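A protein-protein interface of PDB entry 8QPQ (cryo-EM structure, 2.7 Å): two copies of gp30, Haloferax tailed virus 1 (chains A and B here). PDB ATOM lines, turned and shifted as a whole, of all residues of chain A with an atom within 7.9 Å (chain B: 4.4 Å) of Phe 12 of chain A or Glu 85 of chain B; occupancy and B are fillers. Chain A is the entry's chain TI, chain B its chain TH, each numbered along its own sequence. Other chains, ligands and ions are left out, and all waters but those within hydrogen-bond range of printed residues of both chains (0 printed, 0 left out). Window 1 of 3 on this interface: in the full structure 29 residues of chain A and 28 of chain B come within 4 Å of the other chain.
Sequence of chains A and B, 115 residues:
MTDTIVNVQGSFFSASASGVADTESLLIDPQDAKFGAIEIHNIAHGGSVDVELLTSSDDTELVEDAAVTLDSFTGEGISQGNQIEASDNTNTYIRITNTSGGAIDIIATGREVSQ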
ATOM      1  N   GLN A   9      31.245   2.771  15.133  1.00  0.00           N
ATOM      2  CA  GLN A   9      32.058   3.389  14.091  1.00  0.00           C
ATOM      3  C   GLN A   9      31.713   4.873  13.911  1.00  0.00           C
ATOM      4  O   GLN A   9      30.566   5.296  14.062  1.00  0.00           O
ATOM      5  CB  GLN A   9      31.951   2.573  12.808  1.00  0.00           C
ATOM      6  CG  GLN A   9      33.218   2.575  11.970  1.00  0.00           C
ATOM      7  CD  GLN A   9      34.408   1.923  12.626  1.00  0.00           C
ATOM      8  OE1 GLN A   9      34.334   1.279  13.677  1.00  0.00           O
ATOM      9  NE2 GLN A   9      35.544   2.055  11.958  1.00  0.00           N
ATOM     10  N   GLY A  10      32.750   5.640  13.551  1.00  0.00           N
ATOM     11  CA  GLY A  10      32.773   7.098  13.488  1.00  0.00           C
ATOM     12  C   GLY A  10      31.795   7.707  12.490  1.00  0.00           C
ATOM     13  O   GLY A  10      31.203   7.014  11.665  1.00  0.00           O
ATOM     14  N   SER A  11      31.671   9.030  12.568  1.00  0.00           N
ATOM     15  CA  SER A  11      30.519   9.738  12.038  1.00  0.00           C
ATOM     16  C   SER A  11      30.281   9.460  10.561  1.00  0.00           C
ATOM     17  O   SER A  11      31.156   9.636   9.737  1.00  0.00           O
ATOM     18  CB  SER A  11      30.604  11.202  12.322  1.00  0.00           C
ATOM     19  OG  SER A  11      30.511  11.392  13.718  1.00  0.00           O
ATOM     20  N   PHE A  12      29.047   9.073  10.252  1.00  0.00           N
ATOM     21  CA  PHE A  12      28.529   9.005   8.900  1.00  0.00           C
ATOM     22  C   PHE A  12      28.651  10.365   8.207  1.00  0.00           C
ATOM     23  O   PHE A  12      28.421  11.404   8.815  1.00  0.00           O
ATOM     24  CB  PHE A  12      27.076   8.534   8.997  1.00  0.00           C
ATOM     25  CG  PHE A  12      26.312   8.618   7.704  1.00  0.00           C
ATOM     26  CD1 PHE A  12      25.772   9.827   7.295  1.00  0.00           C
ATOM     27  CD2 PHE A  12      26.129   7.502   6.895  1.00  0.00           C
ATOM     28  CE1 PHE A  12      25.121   9.936   6.079  1.00  0.00           C
ATOM     29  CE2 PHE A  12      25.437   7.606   5.695  1.00  0.00           C
ATOM     30  CZ  PHE A  12      24.928   8.824   5.290  1.00  0.00           C
ATOM     31  N   PHE A  13      29.011  10.346   6.922  1.00  0.00           N
ATOM     32  CA  PHE A  13      29.006  11.527   6.077  1.00  0.00           C
ATOM     33  C   PHE A  13      28.264  11.237   4.774  1.00  0.00           C
ATOM     34  O   PHE A  13      28.448  10.175   4.180  1.00  0.00           O
ATOM     35  CB  PHE A  13      30.455  11.943   5.806  1.00  0.00           C
ATOM     36  CG  PHE A  13      30.573  13.176   4.949  1.00  0.00           C
ATOM     37  CD1 PHE A  13      30.513  14.449   5.507  1.00  0.00           C
ATOM     38  CD2 PHE A  13      30.684  13.061   3.570  1.00  0.00           C
ATOM     39  CE1 PHE A  13      30.574  15.587   4.709  1.00  0.00           C
ATOM     40  CE2 PHE A  13      30.737  14.193   2.770  1.00  0.00           C
ATOM     41  CZ  PHE A  13      30.684  15.455   3.340  1.00  0.00           C
ATOM     42  N   SER A  14      27.439  12.182   4.300  1.00  0.00           N
ATOM     43  CA  SER A  14      26.952  12.096   2.929  1.00  0.00           C
ATOM     44  C   SER A  14      26.779  13.459   2.274  1.00  0.00           C
ATOM     45  O   SER A  14      26.522  14.463   2.930  1.00  0.00           O
ATOM     46  CB  SER A  14      25.713  11.258   2.775  1.00  0.00           C
ATOM     47  OG  SER A  14      24.567  11.880   3.326  1.00  0.00           O
ATOM     48  N   ALA A  15      26.936  13.453   0.949  1.00  0.00           N
ATOM     49  CA  ALA A  15      26.594  14.564   0.087  1.00  0.00           C
ATOM     50  C   ALA A  15      25.635  14.043  -0.980  1.00  0.00           C
ATOM     51  O   ALA A  15      25.752  12.910  -1.438  1.00  0.00           O
ATOM     52  CB  ALA A  15      27.855  15.137  -0.504  1.00  0.00           C
ATOM     53  N   ASP A  32      31.963  20.591   5.291  1.00  0.00           N
ATOM     54  CA  ASP A  32      30.645  20.206   5.777  1.00  0.00           C
ATOM     55  C   ASP A  32      30.721  19.137   6.875  1.00  0.00           C
ATOM     56  O   ASP A  32      29.744  18.928   7.602  1.00  0.00           O
ATOM     57  CB  ASP A  32      29.769  19.738   4.614  1.00  0.00           C
ATOM     58  CG  ASP A  32      29.524  20.773   3.526  1.00  0.00           C
ATOM     59  OD1 ASP A  32      29.815  21.952   3.736  1.00  0.00           O
ATOM     60  OD2 ASP A  32      29.000  20.384   2.467  1.00  0.00           O
ATOM     61  N   ALA A  33      31.876  18.475   7.020  1.00  0.00           N
ATOM     62  CA  ALA A  33      32.130  17.501   8.076  1.00  0.00           C
ATOM     63  C   ALA A  33      32.414  18.212   9.404  1.00  0.00           C
ATOM     64  O   ALA A  33      33.047  19.265   9.435  1.00  0.00           O
ATOM     65  CB  ALA A  33      33.301  16.640   7.654  1.00  0.00           C
ATOM     66  N   LYS A  34      32.002  17.606  10.524  1.00  0.00           N
ATOM     67  CA  LYS A  34      32.307  18.110  11.854  1.00  0.00           C
ATOM     68  C   LYS A  34      33.815  18.049  12.136  1.00  0.00           C
ATOM     69  O   LYS A  34      34.387  18.997  12.675  1.00  0.00           O
ATOM     70  CB  LYS A  34      31.481  17.358  12.894  1.00  0.00           C
ATOM     71  CG  LYS A  34      31.568  17.961  14.286  1.00  0.00           C
ATOM     72  CD  LYS A  34      30.696  17.261  15.304  1.00  0.00           C
ATOM     73  CE  LYS A  34      30.569  18.001  16.623  1.00  0.00           C
ATOM     74  NZ  LYS A  34      31.811  17.930  17.433  1.00  0.00           N
ATOM     75  N   ILE A  38      37.013  13.728   5.403  1.00  0.00           N
ATOM     76  CA  ILE A  38      36.066  12.719   4.954  1.00  0.00           C
ATOM     77  C   ILE A  38      36.804  11.638   4.177  1.00  0.00           C
ATOM     78  O   ILE A  38      37.863  11.859   3.586  1.00  0.00           O
ATOM     79  CB  ILE A  38      34.947  13.336   4.095  1.00  0.00           C
ATOM     80  CG1 ILE A  38      35.459  13.825   2.734  1.00  0.00           C
ATOM     81  CG2 ILE A  38      34.213  14.413   4.887  1.00  0.00           C
ATOM     82  CD1 ILE A  38      34.428  14.589   1.912  1.00  0.00           C
ATOM     83  N   GLU A  39      36.170  10.470   4.152  1.00  0.00           N
ATOM     84  CA  GLU A  39      36.569   9.352   3.334  1.00  0.00           C
ATOM     85  C   GLU A  39      35.297   8.856   2.664  1.00  0.00           C
ATOM     86  O   GLU A  39      34.415   8.297   3.319  1.00  0.00           O
ATOM     87  CB  GLU A  39      37.215   8.318   4.257  1.00  0.00           C
ATOM     88  CG  GLU A  39      37.746   7.098   3.563  1.00  0.00           C
ATOM     89  CD  GLU A  39      38.299   6.166   4.640  1.00  0.00           C
ATOM     90  OE1 GLU A  39      37.519   5.541   5.294  1.00  0.00           O
ATOM     91  OE2 GLU A  39      39.551   6.057   4.845  1.00  0.00           O
ATOM     92  N   ILE A  40      35.164   9.097   1.357  1.00  0.00           N
ATOM     93  CA  ILE A  40      34.009   8.637   0.599  1.00  0.00           C
ATOM     94  C   ILE A  40      34.229   7.180   0.207  1.00  0.00           C
ATOM     95  O   ILE A  40      35.234   6.817  -0.375  1.00  0.00           O
ATOM     96  CB  ILE A  40      33.718   9.562  -0.600  1.00  0.00           C
ATOM     97  CG1 ILE A  40      33.300  10.970  -0.145  1.00  0.00           C
ATOM     98  CG2 ILE A  40      32.696   8.960  -1.574  1.00  0.00           C
ATOM     99  CD1 ILE A  40      32.056  11.064   0.706  1.00  0.00           C
ATOM    100  N   HIS A  41      33.255   6.357   0.594  1.00  0.00           N
ATOM    101  CA  HIS A  41      33.233   4.932   0.322  1.00  0.00           C
ATOM    102  C   HIS A  41      32.382   4.644  -0.914  1.00  0.00           C
ATOM    103  O   HIS A  41      32.781   3.899  -1.793  1.00  0.00           O
ATOM    104  CB  HIS A  41      32.674   4.184   1.542  1.00  0.00           C
ATOM    105  CG  HIS A  41      33.474   4.358   2.790  1.00  0.00           C
ATOM    106  ND1 HIS A  41      33.003   4.050   4.061  1.00  0.00           N
ATOM    107  CD2 HIS A  41      34.737   4.791   2.964  1.00  0.00           C
ATOM    108  CE1 HIS A  41      33.958   4.291   4.940  1.00  0.00           C
ATOM    109  NE2 HIS A  41      35.025   4.754   4.288  1.00  0.00           N
ATOM    110  N   ASN A  42      31.226   5.306  -0.971  1.00  0.00           N
ATOM    111  CA  ASN A  42      30.198   4.996  -1.933  1.00  0.00           C
ATOM    112  C   ASN A  42      29.904   6.207  -2.803  1.00  0.00           C
ATOM    113  O   ASN A  42      29.707   7.304  -2.297  1.00  0.00           O
ATOM    114  CB  ASN A  42      28.931   4.620  -1.201  1.00  0.00           C
ATOM    115  CG  ASN A  42      29.062   3.407  -0.316  1.00  0.00           C
ATOM    116  OD1 ASN A  42      29.879   2.499  -0.475  1.00  0.00           O
ATOM    117  ND2 ASN A  42      28.267   3.419   0.729  1.00  0.00           N
ATOM    118  N   ILE A  43      29.864   5.975  -4.116  1.00  0.00           N
ATOM    119  CA  ILE A  43      29.298   6.928  -5.049  1.00  0.00           C
ATOM    120  C   ILE A  43      28.205   6.202  -5.826  1.00  0.00           C
ATOM    121  O   ILE A  43      28.502   5.310  -6.614  1.00  0.00           O
ATOM    122  CB  ILE A  43      30.404   7.499  -5.968  1.00  0.00           C
ATOM    123  CG1 ILE A  43      31.422   8.300  -5.151  1.00  0.00           C
ATOM    124  CG2 ILE A  43      29.800   8.319  -7.106  1.00  0.00           C
ATOM    125  CD1 ILE A  43      32.671   8.696  -5.884  1.00  0.00           C
ATOM    126  N   ILE A  78      26.509   1.872  -8.405  1.00  0.00           N
ATOM    127  CA  ILE A  78      27.261   2.304  -7.244  1.00  0.00           C
ATOM    128  C   ILE A  78      28.702   1.788  -7.289  1.00  0.00           C
ATOM    129  O   ILE A  78      28.959   0.571  -7.360  1.00  0.00           O
ATOM    130  CB  ILE A  78      26.551   1.918  -5.922  1.00  0.00           C
ATOM    131  CG1 ILE A  78      27.289   2.471  -4.700  1.00  0.00           C
ATOM    132  CG2 ILE A  78      26.308   0.408  -5.832  1.00  0.00           C
ATOM    133  CD1 ILE A  78      26.526   2.300  -3.394  1.00  0.00           C
ATOM    134  N   GLN A  80      31.287   1.066  -4.656  1.00  0.00           N
ATOM    135  CA  GLN A  80      31.142   0.806  -3.234  1.00  0.00           C
ATOM    136  C   GLN A  80      32.499   0.441  -2.620  1.00  0.00           C
ATOM    137  O   GLN A  80      33.314  -0.241  -3.238  1.00  0.00           O
ATOM    138  CB  GLN A  80      30.103  -0.307  -3.045  1.00  0.00           C
ATOM    139  CG  GLN A  80      30.042  -0.931  -1.663  1.00  0.00           C
ATOM    140  CD  GLN A  80      28.875  -1.865  -1.524  1.00  0.00           C
ATOM    141  OE1 GLN A  80      28.037  -1.689  -0.642  1.00  0.00           O
ATOM    142  NE2 GLN A  80      28.816  -2.878  -2.377  1.00  0.00           N
ATOM    143  N   GLY A  81      32.760   0.891  -1.375  1.00  0.00           N
ATOM    144  CA  GLY A  81      33.937   0.458  -0.616  1.00  0.00           C
ATOM    145  C   GLY A  81      35.268   1.082  -1.063  1.00  0.00           C
ATOM    146  O   GLY A  81      36.334   0.521  -0.868  1.00  0.00           O
ATOM    147  N   ILE A 107      24.302  10.387  -5.062  1.00  0.00           N
ATOM    148  CA  ILE A 107      24.437  10.253  -3.619  1.00  0.00           C
ATOM    149  C   ILE A 107      25.833   9.698  -3.318  1.00  0.00           C
ATOM    150  O   ILE A 107      26.224   8.644  -3.819  1.00  0.00           O
ATOM    151  CB  ILE A 107      23.316   9.358  -3.038  1.00  0.00           C
ATOM    152  CG1 ILE A 107      21.907   9.815  -3.452  1.00  0.00           C
ATOM    153  CG2 ILE A 107      23.445   9.258  -1.520  1.00  0.00           C
ATOM    154  CD1 ILE A 107      20.806   8.784  -3.240  1.00  0.00           C
ATOM    155  N   ALA A 108      26.596  10.428  -2.503  1.00  0.00           N
ATOM    156  CA  ALA A 108      27.909   9.987  -2.067  1.00  0.00           C
ATOM    157  C   ALA A 108      27.883   9.778  -0.554  1.00  0.00           C
ATOM    158  O   ALA A 108      27.449  10.659   0.182  1.00  0.00           O
ATOM    159  CB  ALA A 108      28.932  11.018  -2.469  1.00  0.00           C
ATOM    160  N   THR A 109      28.325   8.602  -0.081  1.00  0.00           N
ATOM    161  CA  THR A 109      28.385   8.340   1.351  1.00  0.00           C
ATOM    162  C   THR A 109      29.771   7.861   1.766  1.00  0.00           C
ATOM    163  O   THR A 109      30.555   7.335   0.976  1.00  0.00           O
ATOM    164  CB  THR A 109      27.274   7.398   1.849  1.00  0.00           C
ATOM    165  OG1 THR A 109      27.572   6.031   1.558  1.00  0.00           O
ATOM    166  CG2 THR A 109      25.895   7.716   1.313  1.00  0.00           C
ATOM    167  N   GLY A 110      30.071   8.099   3.032  1.00  0.00           N
ATOM    168  CA  GLY A 110      31.324   7.686   3.615  1.00  0.00           C
ATOM    169  C   GLY A 110      31.359   8.038   5.092  1.00  0.00           C
ATOM    170  O   GLY A 110      30.326   8.088   5.758  1.00  0.00           O
ATOM    171  N   ARG A 111      32.558   8.353   5.564  1.00  0.00           N
ATOM    172  CA  ARG A 111      32.807   8.540   6.978  1.00  0.00           C
ATOM    173  C   ARG A 111      33.624   9.805   7.200  1.00  0.00           C
ATOM    174  O   ARG A 111      34.465  10.157   6.386  1.00  0.00           O
ATOM    175  CB  ARG A 111      33.496   7.294   7.535  1.00  0.00           C
ATOM    176  CG  ARG A 111      33.249   7.130   9.035  1.00  0.00           C
ATOM    177  CD  ARG A 111      33.771   5.798   9.545  1.00  0.00           C
ATOM    178  NE  ARG A 111      33.082   4.638   8.997  1.00  0.00           N
ATOM    179  CZ  ARG A 111      33.655   3.484   8.667  1.00  0.00           C
ATOM    180  NH1 ARG A 111      32.908   2.487   8.234  1.00  0.00           N
ATOM    181  NH2 ARG A 111      34.963   3.339   8.719  1.00  0.00           N
ATOM    182  N   GLU A 112      33.379  10.496   8.313  1.00  0.00           N
ATOM    183  CA  GLU A 112      34.260  11.547   8.772  1.00  0.00           C
ATOM    184  C   GLU A 112      35.517  10.964   9.409  1.00  0.00           C
ATOM    185  O   GLU A 112      35.488   9.943  10.098  1.00  0.00           O
ATOM    186  CB  GLU A 112      33.556  12.443   9.783  1.00  0.00           C
ATOM    187  CG  GLU A 112      32.309  13.109   9.230  1.00  0.00           C
ATOM    188  CD  GLU A 112      31.886  14.333  10.022  1.00  0.00           C
ATOM    189  OE1 GLU A 112      32.751  14.952  10.668  1.00  0.00           O
ATOM    190  OE2 GLU A 112      30.729  14.761   9.897  1.00  0.00           O
ATOM    191  N   ALA B  37      22.352   6.079  12.189  1.00  0.00           N
ATOM    192  CA  ALA B  37      22.962   5.742  10.912  1.00  0.00           C
ATOM    193  C   ALA B  37      23.309   4.255  10.877  1.00  0.00           C
ATOM    194  O   ALA B  37      23.520   3.619  11.911  1.00  0.00           O
ATOM    195  CB  ALA B  37      24.171   6.607  10.616  1.00  0.00           C
ATOM    196  N   ILE B  38      23.351   3.705   9.661  1.00  0.00           N
ATOM    197  CA  ILE B  38      23.540   2.283   9.433  1.00  0.00           C
ATOM    198  C   ILE B  38      24.470   2.071   8.246  1.00  0.00           C
ATOM    199  O   ILE B  38      24.582   2.899   7.339  1.00  0.00           O
ATOM    200  CB  ILE B  38      22.197   1.560   9.192  1.00  0.00           C
ATOM    201  CG1 ILE B  38      21.545   1.972   7.867  1.00  0.00           C
ATOM    202  CG2 ILE B  38      21.270   1.766  10.373  1.00  0.00           C
ATOM    203  CD1 ILE B  38      20.190   1.374   7.608  1.00  0.00           C
ATOM    204  N   GLU B  39      25.092   0.903   8.269  1.00  0.00           N
ATOM    205  CA  GLU B  39      25.849   0.360   7.164  1.00  0.00           C
ATOM    206  C   GLU B  39      25.360  -1.073   6.959  1.00  0.00           C
ATOM    207  O   GLU B  39      25.533  -1.889   7.843  1.00  0.00           O
ATOM    208  CB  GLU B  39      27.326   0.473   7.517  1.00  0.00           C
ATOM    209  CG  GLU B  39      28.221  -0.002   6.396  1.00  0.00           C
ATOM    210  CD  GLU B  39      29.688   0.042   6.772  1.00  0.00           C
ATOM    211  OE1 GLU B  39      30.080  -0.541   7.829  1.00  0.00           O
ATOM    212  OE2 GLU B  39      30.444   0.608   6.000  1.00  0.00           O
ATOM    213  N   LEU B  53      18.864   3.358  -3.360  1.00  0.00           N
ATOM    214  CA  LEU B  53      19.253   4.314  -2.339  1.00  0.00           C
ATOM    215  C   LEU B  53      18.513   5.621  -2.597  1.00  0.00           C
ATOM    216  O   LEU B  53      18.549   6.146  -3.705  1.00  0.00           O
ATOM    217  CB  LEU B  53      20.771   4.498  -2.409  1.00  0.00           C
ATOM    218  CG  LEU B  53      21.409   5.314  -1.286  1.00  0.00           C
ATOM    219  CD1 LEU B  53      21.311   4.586   0.046  1.00  0.00           C
ATOM    220  CD2 LEU B  53      22.865   5.594  -1.605  1.00  0.00           C
ATOM    221  N   GLN B  83      28.871  -2.129   1.900  1.00  0.00           N
ATOM    222  CA  GLN B  83      28.954  -1.005   2.821  1.00  0.00           C
ATOM    223  C   GLN B  83      27.930   0.043   2.388  1.00  0.00           C
ATOM    224  O   GLN B  83      28.266   1.201   2.242  1.00  0.00           O
ATOM    225  CB  GLN B  83      30.348  -0.367   2.760  1.00  0.00           C
ATOM    226  CG  GLN B  83      31.500  -1.170   3.359  1.00  0.00           C
ATOM    227  CD  GLN B  83      32.717  -0.289   3.473  1.00  0.00           C
ATOM    228  OE1 GLN B  83      33.670  -0.410   2.704  1.00  0.00           O
ATOM    229  NE2 GLN B  83      32.681   0.626   4.429  1.00  0.00           N
ATOM    230  N   ILE B  84      26.666  -0.324   2.127  1.00  0.00           N
ATOM    231  CA  ILE B  84      25.687   0.679   1.751  1.00  0.00           C
ATOM    232  C   ILE B  84      25.226   1.414   3.008  1.00  0.00           C
ATOM    233  O   ILE B  84      24.893   0.784   4.003  1.00  0.00           O
ATOM    234  CB  ILE B  84      24.561   0.132   0.857  1.00  0.00           C
ATOM    235  CG1 ILE B  84      23.685  -0.925   1.539  1.00  0.00           C
ATOM    236  CG2 ILE B  84      25.151  -0.372  -0.446  1.00  0.00           C
ATOM    237  CD1 ILE B  84      22.549  -1.477   0.689  1.00  0.00           C
ATOM    238  N   GLU B  85      25.318   2.750   2.978  1.00  0.00           N
ATOM    239  CA  GLU B  85      25.174   3.531   4.191  1.00  0.00           C
ATOM    240  C   GLU B  85      23.980   4.476   4.105  1.00  0.00           C
ATOM    241  O   GLU B  85      23.690   5.039   3.056  1.00  0.00           O
ATOM    242  CB  GLU B  85      26.438   4.337   4.474  1.00  0.00           C
ATOM    243  CG  GLU B  85      27.664   3.493   4.724  1.00  0.00           C
ATOM    244  CD  GLU B  85      28.937   4.313   4.556  1.00  0.00           C
ATOM    245  OE1 GLU B  85      29.157   4.890   3.464  1.00  0.00           O
ATOM    246  OE2 GLU B  85      29.671   4.461   5.552  1.00  0.00           O
ATOM    247  N   ALA B  86      23.334   4.684   5.254  1.00  0.00           N
ATOM    248  CA  ALA B  86      22.203   5.588   5.345  1.00  0.00           C
ATOM    249  C   ALA B  86      22.181   6.242   6.729  1.00  0.00           C
ATOM    250  O   ALA B  86      22.546   5.620   7.720  1.00  0.00           O
ATOM    251  CB  ALA B  86      20.955   4.789   5.071  1.00  0.00           C
ATOM    252  N   SER B  87      21.720   7.492   6.814  1.00  0.00           N
ATOM    253  CA  SER B  87      21.496   8.154   8.097  1.00  0.00           C
ATOM    254  C   SER B  87      20.148   8.870   8.119  1.00  0.00           C
ATOM    255  O   SER B  87      19.617   9.266   7.077  1.00  0.00           O
ATOM    256  CB  SER B  87      22.601   9.096   8.488  1.00  0.00           C
ATOM    257  OG  SER B  87      22.412  10.390   7.917  1.00  0.00           O
ATOM    258  N   THR B  90      20.806  12.880   7.299  1.00  0.00           N
ATOM    259  CA  THR B  90      20.926  13.083   5.857  1.00  0.00           C
ATOM    260  C   THR B  90      19.768  12.460   5.076  1.00  0.00           C
ATOM    261  O   THR B  90      19.821  12.381   3.846  1.00  0.00           O
ATOM    262  CB  THR B  90      22.292  12.635   5.317  1.00  0.00           C
ATOM    263  OG1 THR B  90      22.396  11.218   5.309  1.00  0.00           O
ATOM    264  CG2 THR B  90      23.449  13.186   6.111  1.00  0.00           C
ATOM    265  N   THR B  92      18.500   9.567   4.367  1.00  0.00           N
ATOM    266  CA  THR B  92      18.842   8.545   3.390  1.00  0.00           C
ATOM    267  C   THR B  92      18.155   7.239   3.763  1.00  0.00           C
ATOM    268  O   THR B  92      18.192   6.835   4.903  1.00  0.00           O
ATOM    269  CB  THR B  92      20.369   8.415   3.299  1.00  0.00           C
ATOM    270  OG1 THR B  92      20.891   9.658   2.843  1.00  0.00           O
ATOM    271  CG2 THR B  92      20.815   7.413   2.263  1.00  0.00           C
ATOM    272  N   VAL B 113      26.157   3.020  12.846  1.00  0.00           N
ATOM    273  CA  VAL B 113      27.264   3.953  12.714  1.00  0.00           C
ATOM    274  C   VAL B 113      26.843   5.229  13.442  1.00  0.00           C
ATOM    275  O   VAL B 113      25.658   5.542  13.508  1.00  0.00           O
ATOM    276  CB  VAL B 113      27.576   4.190  11.220  1.00  0.00           C
ATOM    277  CG1 VAL B 113      28.771   5.107  11.008  1.00  0.00           C
ATOM    278  CG2 VAL B 113      27.825   2.883  10.478  1.00  0.00           C
ATOM    279  N   SER B 114      27.799   5.956  14.028  1.00  0.00           N
ATOM    280  CA  SER B 114      27.484   7.257  14.596  1.00  0.00           C
ATOM    281  C   SER B 114      27.098   8.237  13.486  1.00  0.00           C
ATOM    282  O   SER B 114      27.628   8.172  12.383  1.00  0.00           O
ATOM    283  CB  SER B 114      28.657   7.790  15.372  1.00  0.00           C
ATOM    284  OG  SER B 114      28.364   9.047  15.955  1.00  0.00           O
ATOM    285  N   GLN B 115      26.179   9.154  13.786  1.00  0.00           N
ATOM    286  CA  GLN B 115      26.077  10.365  12.988  1.00  0.00           C
ATOM    287  C   GLN B 115      27.188  11.353  13.386  1.00  0.00           C
ATOM    288  O   GLN B 115      27.235  12.452  12.766  1.00  0.00           O
ATOM    289  CB  GLN B 115      24.660  10.931  13.063  1.00  0.00           C
ATOM    290  CG  GLN B 115      23.678  10.038  12.325  1.00  0.00           C
ATOM    291  CD  GLN B 115      22.243  10.460  12.487  1.00  0.00           C
ATOM    292  OE1 GLN B 115      21.619  10.890  11.528  1.00  0.00           O
ATOM    293  NE2 GLN B 115      21.698  10.335  13.683  1.00  0.00           N
ATOM    294  OXT GLN B 115      27.998  10.988  14.279  1.00  0.00           O
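N of Phe 12 of chain A lies within hydrogen-bond range of O of Ser 114 of chain B (2.7 Å). NH1 of Arg 111 of chain A lies within salt-bridge range of OE2 of Glu 39 of chain B (3.8 Å). The backbone NH (N) of Ile 84 of chain B sits close to the side-chain amide oxygen (OE1) of Gln 80 of chain A (3.4 Å). O of Gln 83 of chain B sits at hydrogen-bond distance from ND2 of Asn 42 of chain A (2.7 Å). ND2 of Asn 42 of chain A lies within hydrogen-bond range of OE1 of Glu 85 of chain B. The side-chain hydroxyl of Ser 14 of chain A lies within hydrogen-bond range of the side-chain hydroxyl of Thr 90 of chain B (3.0 Å). A ring nitrogen (ND1) of His 41 of chain A lies within hydrogen-bond range of the side-chain amide nitrogen of Gln 83 of chain B, 3.5 Å away. OG1 of Thr 109 of chain A is in hydrogen-bond range of OE1 of Glu 85 of chain B (2.7 Å). The chain-end carboxylate (OXT) of Gln 115 of chain B sits at hydrogen-bond distance from the side-chain hydroxyl (OG) of Ser 11 of chain A. N of Ser 114 of chain B sits at hydrogen-bond distance from O of Gln 9 of chain A, 2.8 Å away. The backbone NH of Gly 110 of chain A sits at hydrogen-bond distance from the side-chain carboxylate of Glu 85 of chain B, 3.4 Å away. The backbone NH of Gln 83 of chain B is in hydrogen-bond range of the side-chain amide oxygen of Gln 80 of chain A (2.7 Å).
The backbone carbonyl oxygen (O) of Arg 111 of chain A lies within hydrogen-bond range of the backbone NH (N) of Glu 39 of chain A, at 2.8 Å. The backbone carbonyl oxygen (O) of Ser 87 of chain B sits at hydrogen-bond distance from the backbone NH (N) of Thr 92 of chain B, at 2.9 Å. O of Thr 109 of chain A lies within hydrogen-bond range of N of His 41 of chain A, at 2.9 Å. The backbone NH (N) of Gly 81 of chain A sits at hydrogen-bond distance from the side-chain amide oxygen (OD1) of Asn 42 of chain A, at 3.4 Å.
Gly 10 of chain A touches Val 113 of chain B (O to CG1, 3.2 Å). Gly 10 of chain A touches Ser 114 of chain B. Ser 11 of chain A touches Ser 114 of chain B (CA to O, 3.3 Å). Ala 37 of chain B touches Phe 12 of chain A. Phe 12 of chain A touches Glu 85 of chain B (CE2 to CB, 3.6 Å). N of Ala 86 of chain B touches CE2 of Phe 12 of chain A, 3.6 Å away. Phe 12 of chain A touches Ser 87 of chain B (CE1 to OG, 3.3 Å). His 41 of chain A touches Glu 85 of chain B. Asn 42 of chain A touches Ile 84 of chain B (ND2 to CA, 3.9 Å). Gln 83 of chain B touches Gly 81 of chain A.
Of the printed residues of chain B, Gly 10 of chain A touches Val 113 (3.2 Å) and Ser 114 (3.8 Å). Of the printed residues of chain B, Ser 11 of chain A touches Ser 114 and Gln 115. Of the printed residues of chain B, Phe 12 of chain A touches Ala 37, Glu 85, Ala 86, Ser 87, Thr 90 and Ser 114. Of the printed residues of chain B, Ser 14 of chain A touches Thr 90 (3.0 Å). Of the printed residues of chain A, Gln 83 of chain B touches His 41 (3.5 Å), Asn 42 (2.7 Å), Gln 80 (2.7 Å) and Gly 81 (3.4 Å). Of chain A, only Phe 12, His 41, Asn 42, Thr 109 and Gly 110 come within 4 Å of Glu 85 of chain B. Of the printed residues of chain A, Ser 114 of chain B touches Gln 9, Gly 10, Ser 11 and Phe 12. The nearest residue of chain B that does not touch Phe 12 of chain A is Val 113 of chain B (4.05 Å). The nearest residue of chain A that does not touch Glu 85 of chain B is Arg 111 of chain A (4.6 Å).
Hydrophobic or aromatic side chains of chain A within 4 Å of the printed part of chain B: Phe 12, His 41 and Ile 107. Among the printed residues, 25 pairs touch across the chains. Among the printed residues, Asp or Glu carboxylates within 4 Å of a Lys or Arg side-chain nitrogen of the other chain: Arg 111 of chain A with Glu 39 of chain B (3.8 Å).
Positions printed for both chains: 38 and 39. Of the 25 pairs that touch across the chains among the printed residues, none has its exchanged pair printed and touching as well.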
